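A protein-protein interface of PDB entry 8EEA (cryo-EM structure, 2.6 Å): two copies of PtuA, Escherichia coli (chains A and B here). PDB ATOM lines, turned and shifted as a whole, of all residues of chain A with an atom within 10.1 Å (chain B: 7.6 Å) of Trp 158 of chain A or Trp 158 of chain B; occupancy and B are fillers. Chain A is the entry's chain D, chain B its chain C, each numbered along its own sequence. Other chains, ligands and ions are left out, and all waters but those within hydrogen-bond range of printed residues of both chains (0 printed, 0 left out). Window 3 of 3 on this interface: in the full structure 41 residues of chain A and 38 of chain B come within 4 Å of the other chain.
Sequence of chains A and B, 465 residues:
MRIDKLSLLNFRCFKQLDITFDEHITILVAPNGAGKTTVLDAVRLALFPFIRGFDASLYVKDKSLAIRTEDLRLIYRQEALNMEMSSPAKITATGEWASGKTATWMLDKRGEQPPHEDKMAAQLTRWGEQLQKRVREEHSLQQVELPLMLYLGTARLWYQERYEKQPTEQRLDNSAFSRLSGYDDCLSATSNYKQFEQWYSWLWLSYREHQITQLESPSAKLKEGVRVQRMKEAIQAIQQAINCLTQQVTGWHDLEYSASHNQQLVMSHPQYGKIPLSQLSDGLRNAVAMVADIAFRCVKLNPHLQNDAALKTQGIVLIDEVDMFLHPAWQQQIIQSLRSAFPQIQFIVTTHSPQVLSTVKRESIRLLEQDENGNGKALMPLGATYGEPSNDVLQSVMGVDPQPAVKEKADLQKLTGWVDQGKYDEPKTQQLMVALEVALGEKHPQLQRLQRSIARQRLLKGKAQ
Trp 158 of chain A touches Leu 157 of chain B, but with the chains exchanged Leu 157 of chain A does not touch Trp 158 of chain B (6.6 Å).
Trp 158 of chain A touches its own counterpart, Trp 158 of chain B.
Tyr 159 of chain A touches Trp 158 of chain B, but with the chains exchanged Trp 158 of chain A does not touch Tyr 159 of chain B (4.4 Å).
Positions printed for both chains: 154, 155, 156, 157, 158, 159, 190, 191, 192 and 325.
Among the printed residues, merely in contact across the chains: Trp 158 of chain A with Trp 158 of chain B, Trp 158 of chain A with Leu 157 of chain B, Met 324 of chain A with Phe 325 of chain B and Tyr 159 of chain A with Trp 158 of chain B.
The side-chain amide nitrogen of Asn 286 of chain A lies within hydrogen-bond range of the backbone carbonyl oxygen of Met 324 of chain A, 3.3 Å away.
The backbone carbonyl oxygen (O) of Tyr 159 of chain A sits close to the guanidinium group (NE) of Arg 162 of chain A (3.5 Å).
Of the 10 printed residues of chain B, 3 touch a printed residue of chain A.
Printed residues of chain B that touch a printed residue of chain A: Leu 157, Trp 158 and Phe 325.
Hydrophobic or aromatic side chains of chain B within 4 Å of the printed part of chain A: Trp 158 and Phe 325.
Of the 20 printed residues of chain A, 3 touch a printed residue of chain B.
Printed residues of chain A that touch a printed residue of chain B: Trp 158, Tyr 159 and Met 324.
Hydrophobic or aromatic side chains of chain A within 4 Å of the printed part of chain B: Trp 158, Tyr 159 and Met 324.
Trp 158 of chain A touches just these residues of chain B: Leu 157 and Trp 158.
Printed residues of chain B within 4 Å of Tyr 159 of chain A: Trp 158.
Ala 289 of chain A touches none of the printed residues of chain B.
Printed residues of chain B within 4 Å of Met 324 of chain A: Phe 325.
Thr 154 of chain B touches none of the printed residues of chain A.
Leu 157 of chain B touches just one residue of chain A: Trp 158 (3.3 Å).
Trp 158 of chain B touches just these residues of chain A: Trp 158 (3.0 Å) and Tyr 159 (3.8 Å).
Printed residues of chain A within 4 Å of Phe 325 of chain B: Met 324 (3.5 Å).
The nearest residue of chain B that does not touch Trp 158 of chain A is Tyr 159 of chain B (4.4 Å).
The nearest residue of chain A that does not touch Trp 158 of chain B is Leu 157 of chain A (6.6 Å).
The nearest printed residue of chain B that does not touch Tyr 159 of chain A is Ala 155 of chain B (8.3 Å).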
ATOM      1  N   GLY A 153      -4.480   0.705  26.695  1.00  0.00           N
ATOM      2  CA  GLY A 153      -3.582   1.048  27.776  1.00  0.00           C
ATOM      3  C   GLY A 153      -2.125   0.830  27.412  1.00  0.00           C
ATOM      4  O   GLY A 153      -1.778   0.428  26.301  1.00  0.00           O
ATOM      5  N   THR A 154      -1.255   1.105  28.387  1.00  0.00           N
ATOM      6  CA  THR A 154       0.179   0.928  28.181  1.00  0.00           C
ATOM      7  C   THR A 154       0.572  -0.538  28.088  1.00  0.00           C
ATOM      8  O   THR A 154       1.643  -0.846  27.556  1.00  0.00           O
ATOM      9  CB  THR A 154       0.969   1.586  29.312  1.00  0.00           C
ATOM     10  OG1 THR A 154       0.637   0.965  30.559  1.00  0.00           O
ATOM     11  CG2 THR A 154       0.655   3.061  29.390  1.00  0.00           C
ATOM     12  N   ALA A 155      -0.265  -1.447  28.590  1.00  0.00           N
ATOM     13  CA  ALA A 155       0.016  -2.876  28.569  1.00  0.00           C
ATOM     14  C   ALA A 155      -0.550  -3.564  27.334  1.00  0.00           C
ATOM     15  O   ALA A 155      -0.859  -4.759  27.385  1.00  0.00           O
ATOM     16  CB  ALA A 155      -0.529  -3.533  29.836  1.00  0.00           C
ATOM     17  N   ARG A 156      -0.693  -2.842  26.224  1.00  0.00           N
ATOM     18  CA  ARG A 156      -1.264  -3.416  25.014  1.00  0.00           C
ATOM     19  C   ARG A 156      -0.238  -4.155  24.164  1.00  0.00           C
ATOM     20  O   ARG A 156      -0.587  -4.628  23.078  1.00  0.00           O
ATOM     21  CB  ARG A 156      -1.936  -2.320  24.177  1.00  0.00           C
ATOM     22  CG  ARG A 156      -1.003  -1.230  23.665  1.00  0.00           C
ATOM     23  CD  ARG A 156      -1.776  -0.206  22.846  1.00  0.00           C
ATOM     24  NE  ARG A 156      -0.953   0.916  22.407  1.00  0.00           N
ATOM     25  CZ  ARG A 156      -0.772   2.037  23.092  1.00  0.00           C
ATOM     26  NH1 ARG A 156      -1.305   2.214  24.288  1.00  0.00           N
ATOM     27  NH2 ARG A 156      -0.033   3.008  22.562  1.00  0.00           N
ATOM     28  N   LEU A 157       1.011  -4.266  24.623  1.00  0.00           N
ATOM     29  CA  LEU A 157       2.051  -4.980  23.894  1.00  0.00           C
ATOM     30  C   LEU A 157       2.800  -5.973  24.775  1.00  0.00           C
ATOM     31  O   LEU A 157       3.842  -6.488  24.356  1.00  0.00           O
ATOM     32  CB  LEU A 157       3.057  -3.998  23.286  1.00  0.00           C
ATOM     33  CG  LEU A 157       2.500  -2.942  22.335  1.00  0.00           C
ATOM     34  CD1 LEU A 157       3.549  -1.879  22.075  1.00  0.00           C
ATOM     35  CD2 LEU A 157       2.035  -3.578  21.038  1.00  0.00           C
ATOM     36  N   TRP A 158       2.296  -6.259  25.974  1.00  0.00           N
ATOM     37  CA  TRP A 158       3.098  -6.957  26.972  1.00  0.00           C
ATOM     38  C   TRP A 158       3.261  -8.433  26.626  1.00  0.00           C
ATOM     39  O   TRP A 158       4.386  -8.932  26.502  1.00  0.00           O
ATOM     40  CB  TRP A 158       2.458  -6.788  28.349  1.00  0.00           C
ATOM     41  CG  TRP A 158       2.960  -5.590  29.095  1.00  0.00           C
ATOM     42  CD1 TRP A 158       3.591  -4.500  28.569  1.00  0.00           C
ATOM     43  CD2 TRP A 158       2.868  -5.357  30.503  1.00  0.00           C
ATOM     44  NE1 TRP A 158       3.898  -3.605  29.561  1.00  0.00           N
ATOM     45  CE2 TRP A 158       3.463  -4.106  30.760  1.00  0.00           C
ATOM     46  CE3 TRP A 158       2.339  -6.083  31.573  1.00  0.00           C
ATOM     47  CZ2 TRP A 158       3.547  -3.570  32.040  1.00  0.00           C
ATOM     48  CZ3 TRP A 158       2.423  -5.547  32.843  1.00  0.00           C
ATOM     49  CH2 TRP A 158       3.021  -4.303  33.065  1.00  0.00           C
ATOM     50  N   TYR A 159       2.152  -9.149  26.472  1.00  0.00           N
ATOM     51  CA  TYR A 159       2.170 -10.592  26.254  1.00  0.00           C
ATOM     52  C   TYR A 159       1.375 -10.944  25.007  1.00  0.00           C
ATOM     53  O   TYR A 159       0.495 -11.803  25.019  1.00  0.00           O
ATOM     54  CB  TYR A 159       1.630 -11.342  27.471  1.00  0.00           C
ATOM     55  CG  TYR A 159       1.922 -12.833  27.479  1.00  0.00           C
ATOM     56  CD1 TYR A 159       2.923 -13.378  26.680  1.00  0.00           C
ATOM     57  CD2 TYR A 159       1.195 -13.696  28.289  1.00  0.00           C
ATOM     58  CE1 TYR A 159       3.188 -14.735  26.688  1.00  0.00           C
ATOM     59  CE2 TYR A 159       1.455 -15.056  28.303  1.00  0.00           C
ATOM     60  CZ  TYR A 159       2.452 -15.568  27.500  1.00  0.00           C
ATOM     61  OH  TYR A 159       2.715 -16.919  27.508  1.00  0.00           O
ATOM     62  N   GLN A 160       1.685 -10.264  23.901  1.00  0.00           N
ATOM     63  CA  GLN A 160       0.932 -10.448  22.663  1.00  0.00           C
ATOM     64  C   GLN A 160       0.650 -11.915  22.356  1.00  0.00           C
ATOM     65  O   GLN A 160      -0.326 -12.222  21.663  1.00  0.00           O
ATOM     66  CB  GLN A 160       1.695  -9.818  21.498  1.00  0.00           C
ATOM     67  CG  GLN A 160       1.515  -8.318  21.375  1.00  0.00           C
ATOM     68  CD  GLN A 160       2.033  -7.778  20.058  1.00  0.00           C
ATOM     69  OE1 GLN A 160       2.693  -8.489  19.302  1.00  0.00           O
ATOM     70  NE2 GLN A 160       1.736  -6.516  19.778  1.00  0.00           N
ATOM     71  N   GLU A 161       1.483 -12.833  22.849  1.00  0.00           N
ATOM     72  CA  GLU A 161       1.341 -14.256  22.543  1.00  0.00           C
ATOM     73  C   GLU A 161       0.675 -14.986  23.710  1.00  0.00           C
ATOM     74  O   GLU A 161       1.324 -15.618  24.542  1.00  0.00           O
ATOM     75  CB  GLU A 161       2.701 -14.859  22.206  1.00  0.00           C
ATOM     76  CG  GLU A 161       3.571 -13.963  21.339  1.00  0.00           C
ATOM     77  CD  GLU A 161       4.793 -14.677  20.798  1.00  0.00           C
ATOM     78  OE1 GLU A 161       4.798 -15.924  20.778  1.00  0.00           O
ATOM     79  OE2 GLU A 161       5.753 -13.986  20.395  1.00  0.00           O
ATOM     80  N   ARG A 162      -0.656 -14.894  23.758  1.00  0.00           N
ATOM     81  CA  ARG A 162      -1.464 -15.799  24.571  1.00  0.00           C
ATOM     82  C   ARG A 162      -2.934 -15.649  24.197  1.00  0.00           C
ATOM     83  O   ARG A 162      -3.460 -14.533  24.158  1.00  0.00           O
ATOM     84  CB  ARG A 162      -1.258 -15.553  26.074  1.00  0.00           C
ATOM     85  CG  ARG A 162      -2.102 -14.440  26.698  1.00  0.00           C
ATOM     86  CD  ARG A 162      -1.664 -13.071  26.236  1.00  0.00           C
ATOM     87  NE  ARG A 162      -2.437 -12.003  26.857  1.00  0.00           N
ATOM     88  CZ  ARG A 162      -3.590 -11.540  26.394  1.00  0.00           C
ATOM     89  NH1 ARG A 162      -4.136 -12.021  25.288  1.00  0.00           N
ATOM     90  NH2 ARG A 162      -4.209 -10.569  27.055  1.00  0.00           N
ATOM     91  N   ALA A 189      -7.931  -4.061  29.835  1.00  0.00           N
ATOM     92  CA  ALA A 189      -6.623  -3.453  30.027  1.00  0.00           C
ATOM     93  C   ALA A 189      -5.481  -4.299  29.480  1.00  0.00           C
ATOM     94  O   ALA A 189      -4.320  -3.918  29.644  1.00  0.00           O
ATOM     95  CB  ALA A 189      -6.388  -3.182  31.516  1.00  0.00           C
ATOM     96  N   THR A 190      -5.774  -5.421  28.833  1.00  0.00           N
ATOM     97  CA  THR A 190      -4.762  -6.340  28.332  1.00  0.00           C
ATOM     98  C   THR A 190      -4.700  -6.282  26.807  1.00  0.00           C
ATOM     99  O   THR A 190      -5.502  -5.620  26.145  1.00  0.00           O
ATOM    100  CB  THR A 190      -5.051  -7.762  28.812  1.00  0.00           C
ATOM    101  OG1 THR A 190      -6.402  -8.114  28.492  1.00  0.00           O
ATOM    102  CG2 THR A 190      -4.844  -7.871  30.312  1.00  0.00           C
ATOM    103  N   SER A 191      -3.727  -6.999  26.250  1.00  0.00           N
ATOM    104  CA  SER A 191      -3.526  -7.017  24.810  1.00  0.00           C
ATOM    105  C   SER A 191      -4.644  -7.779  24.107  1.00  0.00           C
ATOM    106  O   SER A 191      -5.155  -8.783  24.609  1.00  0.00           O
ATOM    107  CB  SER A 191      -2.176  -7.651  24.475  1.00  0.00           C
ATOM    108  OG  SER A 191      -1.880  -7.523  23.096  1.00  0.00           O
ATOM    109  N   ASN A 192      -5.019  -7.287  22.924  1.00  0.00           N
ATOM    110  CA  ASN A 192      -6.064  -7.889  22.105  1.00  0.00           C
ATOM    111  C   ASN A 192      -5.538  -8.296  20.732  1.00  0.00           C
ATOM    112  O   ASN A 192      -6.298  -8.306  19.758  1.00  0.00           O
ATOM    113  CB  ASN A 192      -7.240  -6.921  21.955  1.00  0.00           C
ATOM    114  CG  ASN A 192      -8.254  -7.055  23.071  1.00  0.00           C
ATOM    115  OD1 ASN A 192      -8.890  -8.096  23.228  1.00  0.00           O
ATOM    116  ND2 ASN A 192      -8.417  -5.993  23.850  1.00  0.00           N
ATOM    117  N   TYR A 193      -4.251  -8.630  20.632  1.00  0.00           N
ATOM    118  CA  TYR A 193      -3.629  -8.866  19.335  1.00  0.00           C
ATOM    119  C   TYR A 193      -3.981 -10.226  18.739  1.00  0.00           C
ATOM    120  O   TYR A 193      -4.141 -10.338  17.518  1.00  0.00           O
ATOM    121  CB  TYR A 193      -2.112  -8.731  19.459  1.00  0.00           C
ATOM    122  CG  TYR A 193      -1.374  -9.026  18.176  1.00  0.00           C
ATOM    123  CD1 TYR A 193      -1.376  -8.119  17.128  1.00  0.00           C
ATOM    124  CD2 TYR A 193      -0.679 -10.216  18.013  1.00  0.00           C
ATOM    125  CE1 TYR A 193      -0.708  -8.388  15.952  1.00  0.00           C
ATOM    126  CE2 TYR A 193      -0.011 -10.493  16.843  1.00  0.00           C
ATOM    127  CZ  TYR A 193      -0.026  -9.576  15.817  1.00  0.00           C
ATOM    128  OH  TYR A 193       0.643  -9.852  14.648  1.00  0.00           O
ATOM    129  N   ARG A 285       5.248  -2.207  15.020  1.00  0.00           N
ATOM    130  CA  ARG A 285       4.332  -3.186  15.595  1.00  0.00           C
ATOM    131  C   ARG A 285       3.315  -2.516  16.513  1.00  0.00           C
ATOM    132  O   ARG A 285       2.119  -2.839  16.472  1.00  0.00           O
ATOM    133  CB  ARG A 285       5.127  -4.254  16.343  1.00  0.00           C
ATOM    134  CG  ARG A 285       6.017  -5.090  15.434  1.00  0.00           C
ATOM    135  CD  ARG A 285       6.543  -6.337  16.124  1.00  0.00           C
ATOM    136  NE  ARG A 285       7.847  -6.117  16.740  1.00  0.00           N
ATOM    137  CZ  ARG A 285       8.041  -5.841  18.024  1.00  0.00           C
ATOM    138  NH1 ARG A 285       7.033  -5.733  18.872  1.00  0.00           N
ATOM    139  NH2 ARG A 285       9.283  -5.668  18.468  1.00  0.00           N
ATOM    140  N   ASN A 286       3.770  -1.575  17.343  1.00  0.00           N
ATOM    141  CA  ASN A 286       2.853  -0.831  18.200  1.00  0.00           C
ATOM    142  C   ASN A 286       1.777  -0.130  17.380  1.00  0.00           C
ATOM    143  O   ASN A 286       0.579  -0.248  17.670  1.00  0.00           O
ATOM    144  CB  ASN A 286       3.637   0.187  19.027  1.00  0.00           C
ATOM    145  CG  ASN A 286       2.760   0.954  19.990  1.00  0.00           C
ATOM    146  OD1 ASN A 286       1.547   0.756  20.040  1.00  0.00           O
ATOM    147  ND2 ASN A 286       3.368   1.848  20.755  1.00  0.00           N
ATOM    148  N   ALA A 289      -0.733  -2.603  15.693  1.00  0.00           N
ATOM    149  CA  ALA A 289      -1.708  -3.127  16.645  1.00  0.00           C
ATOM    150  C   ALA A 289      -2.748  -2.070  16.992  1.00  0.00           C
ATOM    151  O   ALA A 289      -3.961  -2.338  16.989  1.00  0.00           O
ATOM    152  CB  ALA A 289      -0.995  -3.616  17.905  1.00  0.00           C
ATOM    153  N   MET A 324       4.304   6.052  21.937  1.00  0.00           N
ATOM    154  CA  MET A 324       5.367   5.178  22.417  1.00  0.00           C
ATOM    155  C   MET A 324       6.156   4.600  21.251  1.00  0.00           C
ATOM    156  O   MET A 324       5.580   4.185  20.241  1.00  0.00           O
ATOM    157  CB  MET A 324       4.798   4.040  23.263  1.00  0.00           C
ATOM    158  CG  MET A 324       4.188   4.475  24.575  1.00  0.00           C
ATOM    159  SD  MET A 324       3.602   3.078  25.556  1.00  0.00           S
ATOM    160  CE  MET A 324       2.110   2.633  24.675  1.00  0.00           C
ATOM    161  N   PHE A 325       7.479   4.571  21.395  1.00  0.00           N
ATOM    162  CA  PHE A 325       8.412   3.935  20.470  1.00  0.00           C
ATOM    163  C   PHE A 325       8.536   4.673  19.144  1.00  0.00           C
ATOM    164  O   PHE A 325       9.320   4.252  18.287  1.00  0.00           O
ATOM    165  CB  PHE A 325       8.023   2.475  20.200  1.00  0.00           C
ATOM    166  CG  PHE A 325       8.102   1.590  21.414  1.00  0.00           C
ATOM    167  CD1 PHE A 325       9.184   1.658  22.271  1.00  0.00           C
ATOM    168  CD2 PHE A 325       7.092   0.687  21.694  1.00  0.00           C
ATOM    169  CE1 PHE A 325       9.255   0.850  23.385  1.00  0.00           C
ATOM    170  CE2 PHE A 325       7.160  -0.124  22.807  1.00  0.00           C
ATOM    171  CZ  PHE A 325       8.244  -0.043  23.652  1.00  0.00           C
ATOM    172  N   THR B 154      13.304  -3.738  25.917  1.00  0.00           N
ATOM    173  CA  THR B 154      12.038  -3.020  25.968  1.00  0.00           C
ATOM    174  C   THR B 154      10.966  -3.775  26.742  1.00  0.00           C
ATOM    175  O   THR B 154       9.930  -3.183  27.065  1.00  0.00           O
ATOM    176  CB  THR B 154      11.534  -2.732  24.552  1.00  0.00           C
ATOM    177  OG1 THR B 154      11.512  -3.945  23.793  1.00  0.00           O
ATOM    178  CG2 THR B 154      12.430  -1.720  23.859  1.00  0.00           C
ATOM    179  N   ALA B 155      11.185  -5.053  27.045  1.00  0.00           N
ATOM    180  CA  ALA B 155      10.247  -5.857  27.814  1.00  0.00           C
ATOM    181  C   ALA B 155      10.597  -5.895  29.296  1.00  0.00           C
ATOM    182  O   ALA B 155      10.122  -6.778  30.016  1.00  0.00           O
ATOM    183  CB  ALA B 155      10.190  -7.276  27.253  1.00  0.00           C
ATOM    184  N   ARG B 156      11.415  -4.955  29.765  1.00  0.00           N
ATOM    185  CA  ARG B 156      11.879  -4.962  31.148  1.00  0.00           C
ATOM    186  C   ARG B 156      10.806  -4.543  32.144  1.00  0.00           C
ATOM    187  O   ARG B 156      11.119  -4.412  33.330  1.00  0.00           O
ATOM    188  CB  ARG B 156      13.101  -4.053  31.291  1.00  0.00           C
ATOM    189  CG  ARG B 156      12.866  -2.592  30.933  1.00  0.00           C
ATOM    190  CD  ARG B 156      14.155  -1.791  31.047  1.00  0.00           C
ATOM    191  NE  ARG B 156      13.951  -0.364  30.821  1.00  0.00           N
ATOM    192  CZ  ARG B 156      14.302   0.293  29.722  1.00  0.00           C
ATOM    193  NH1 ARG B 156      14.874  -0.318  28.697  1.00  0.00           N
ATOM    194  NH2 ARG B 156      14.068   1.599  29.645  1.00  0.00           N
ATOM    195  N   LEU B 157       9.564  -4.329  31.706  1.00  0.00           N
ATOM    196  CA  LEU B 157       8.469  -4.003  32.607  1.00  0.00           C
ATOM    197  C   LEU B 157       7.305  -4.979  32.535  1.00  0.00           C
ATOM    198  O   LEU B 157       6.347  -4.819  33.300  1.00  0.00           O
ATOM    199  CB  LEU B 157       7.934  -2.592  32.317  1.00  0.00           C
ATOM    200  CG  LEU B 157       8.933  -1.439  32.385  1.00  0.00           C
ATOM    201  CD1 LEU B 157       8.280  -0.158  31.906  1.00  0.00           C
ATOM    202  CD2 LEU B 157       9.469  -1.274  33.792  1.00  0.00           C
ATOM    203  N   TRP B 158       7.351  -5.978  31.652  1.00  0.00           N
ATOM    204  CA  TRP B 158       6.177  -6.814  31.425  1.00  0.00           C
ATOM    205  C   TRP B 158       5.764  -7.549  32.694  1.00  0.00           C
ATOM    206  O   TRP B 158       4.578  -7.593  33.040  1.00  0.00           O
ATOM    207  CB  TRP B 158       6.450  -7.813  30.298  1.00  0.00           C
ATOM    208  CG  TRP B 158       5.588  -9.044  30.370  1.00  0.00           C
ATOM    209  CD1 TRP B 158       4.224  -9.087  30.407  1.00  0.00           C
ATOM    210  CD2 TRP B 158       6.032 -10.406  30.416  1.00  0.00           C
ATOM    211  NE1 TRP B 158       3.791 -10.388  30.472  1.00  0.00           N
ATOM    212  CE2 TRP B 158       4.881 -11.218  30.480  1.00  0.00           C
ATOM    213  CE3 TRP B 158       7.289 -11.018  30.411  1.00  0.00           C
ATOM    214  CZ2 TRP B 158       4.951 -12.607  30.536  1.00  0.00           C
ATOM    215  CZ3 TRP B 158       7.355 -12.398  30.467  1.00  0.00           C
ATOM    216  CH2 TRP B 158       6.193 -13.177  30.529  1.00  0.00           C
ATOM    217  N   TYR B 159       6.723  -8.133  33.400  1.00  0.00           N
ATOM    218  CA  TYR B 159       6.388  -8.971  34.546  1.00  0.00           C
ATOM    219  C   TYR B 159       5.814  -8.135  35.682  1.00  0.00           C
ATOM    220  O   TYR B 159       4.601  -7.944  35.774  1.00  0.00           O
ATOM    221  CB  TYR B 159       7.617  -9.745  35.027  1.00  0.00           C
ATOM    222  CG  TYR B 159       7.273 -10.997  35.803  1.00  0.00           C
ATOM    223  CD1 TYR B 159       6.562 -12.031  35.209  1.00  0.00           C
ATOM    224  CD2 TYR B 159       7.653 -11.141  37.129  1.00  0.00           C
ATOM    225  CE1 TYR B 159       6.243 -13.177  35.913  1.00  0.00           C
ATOM    226  CE2 TYR B 159       7.339 -12.284  37.843  1.00  0.00           C
ATOM    227  CZ  TYR B 159       6.633 -13.297  37.230  1.00  0.00           C
ATOM    228  OH  TYR B 159       6.318 -14.436  37.935  1.00  0.00           O
ATOM    229  N   THR B 190      14.649  -8.315  34.224  1.00  0.00           N
ATOM    230  CA  THR B 190      13.433  -7.526  34.352  1.00  0.00           C
ATOM    231  C   THR B 190      13.573  -6.593  35.546  1.00  0.00           C
ATOM    232  O   THR B 190      14.286  -6.897  36.505  1.00  0.00           O
ATOM    233  CB  THR B 190      12.195  -8.420  34.532  1.00  0.00           C
ATOM    234  OG1 THR B 190      12.134  -9.379  33.470  1.00  0.00           O
ATOM    235  CG2 THR B 190      10.923  -7.589  34.529  1.00  0.00           C
ATOM    236  N   SER B 191      12.894  -5.447  35.479  1.00  0.00           N
ATOM    237  CA  SER B 191      12.977  -4.457  36.553  1.00  0.00           C
ATOM    238  C   SER B 191      11.700  -3.622  36.537  1.00  0.00           C
ATOM    239  O   SER B 191      11.565  -2.706  35.719  1.00  0.00           O
ATOM    240  CB  SER B 191      14.213  -3.583  36.392  1.00  0.00           C
ATOM    241  OG  SER B 191      13.973  -2.518  35.491  1.00  0.00           O
ATOM    242  N   ASN B 192      10.780  -3.934  37.446  1.00  0.00           N
ATOM    243  CA  ASN B 192       9.607  -3.112  37.699  1.00  0.00           C
ATOM    244  C   ASN B 192       9.508  -2.858  39.197  1.00  0.00           C
ATOM    245  O   ASN B 192      10.037  -3.621  40.011  1.00  0.00           O
ATOM    246  CB  ASN B 192       8.323  -3.765  37.170  1.00  0.00           C
ATOM    247  CG  ASN B 192       8.106  -5.155  37.721  1.00  0.00           C
ATOM    248  OD1 ASN B 192       8.863  -5.629  38.565  1.00  0.00           O
ATOM    249  ND2 ASN B 192       7.064  -5.821  37.241  1.00  0.00           N
ATOM    250  N   PHE B 325       9.222   6.440  28.904  1.00  0.00           N
ATOM    251  CA  PHE B 325       8.287   7.009  29.873  1.00  0.00           C
ATOM    252  C   PHE B 325       8.944   8.073  30.746  1.00  0.00           C
ATOM    253  O   PHE B 325       8.554   8.271  31.897  1.00  0.00           O
ATOM    254  CB  PHE B 325       7.676   5.914  30.751  1.00  0.00           C
ATOM    255  CG  PHE B 325       6.882   4.896  29.987  1.00  0.00           C
ATOM    256  CD1 PHE B 325       5.809   5.278  29.202  1.00  0.00           C
ATOM    257  CD2 PHE B 325       7.208   3.553  30.055  1.00  0.00           C
ATOM    258  CE1 PHE B 325       5.081   4.342  28.499  1.00  0.00           C
ATOM    259  CE2 PHE B 325       6.481   2.614  29.353  1.00  0.00           C
ATOM    260  CZ  PHE B 325       5.418   3.011  28.575  1.00  0.00           C
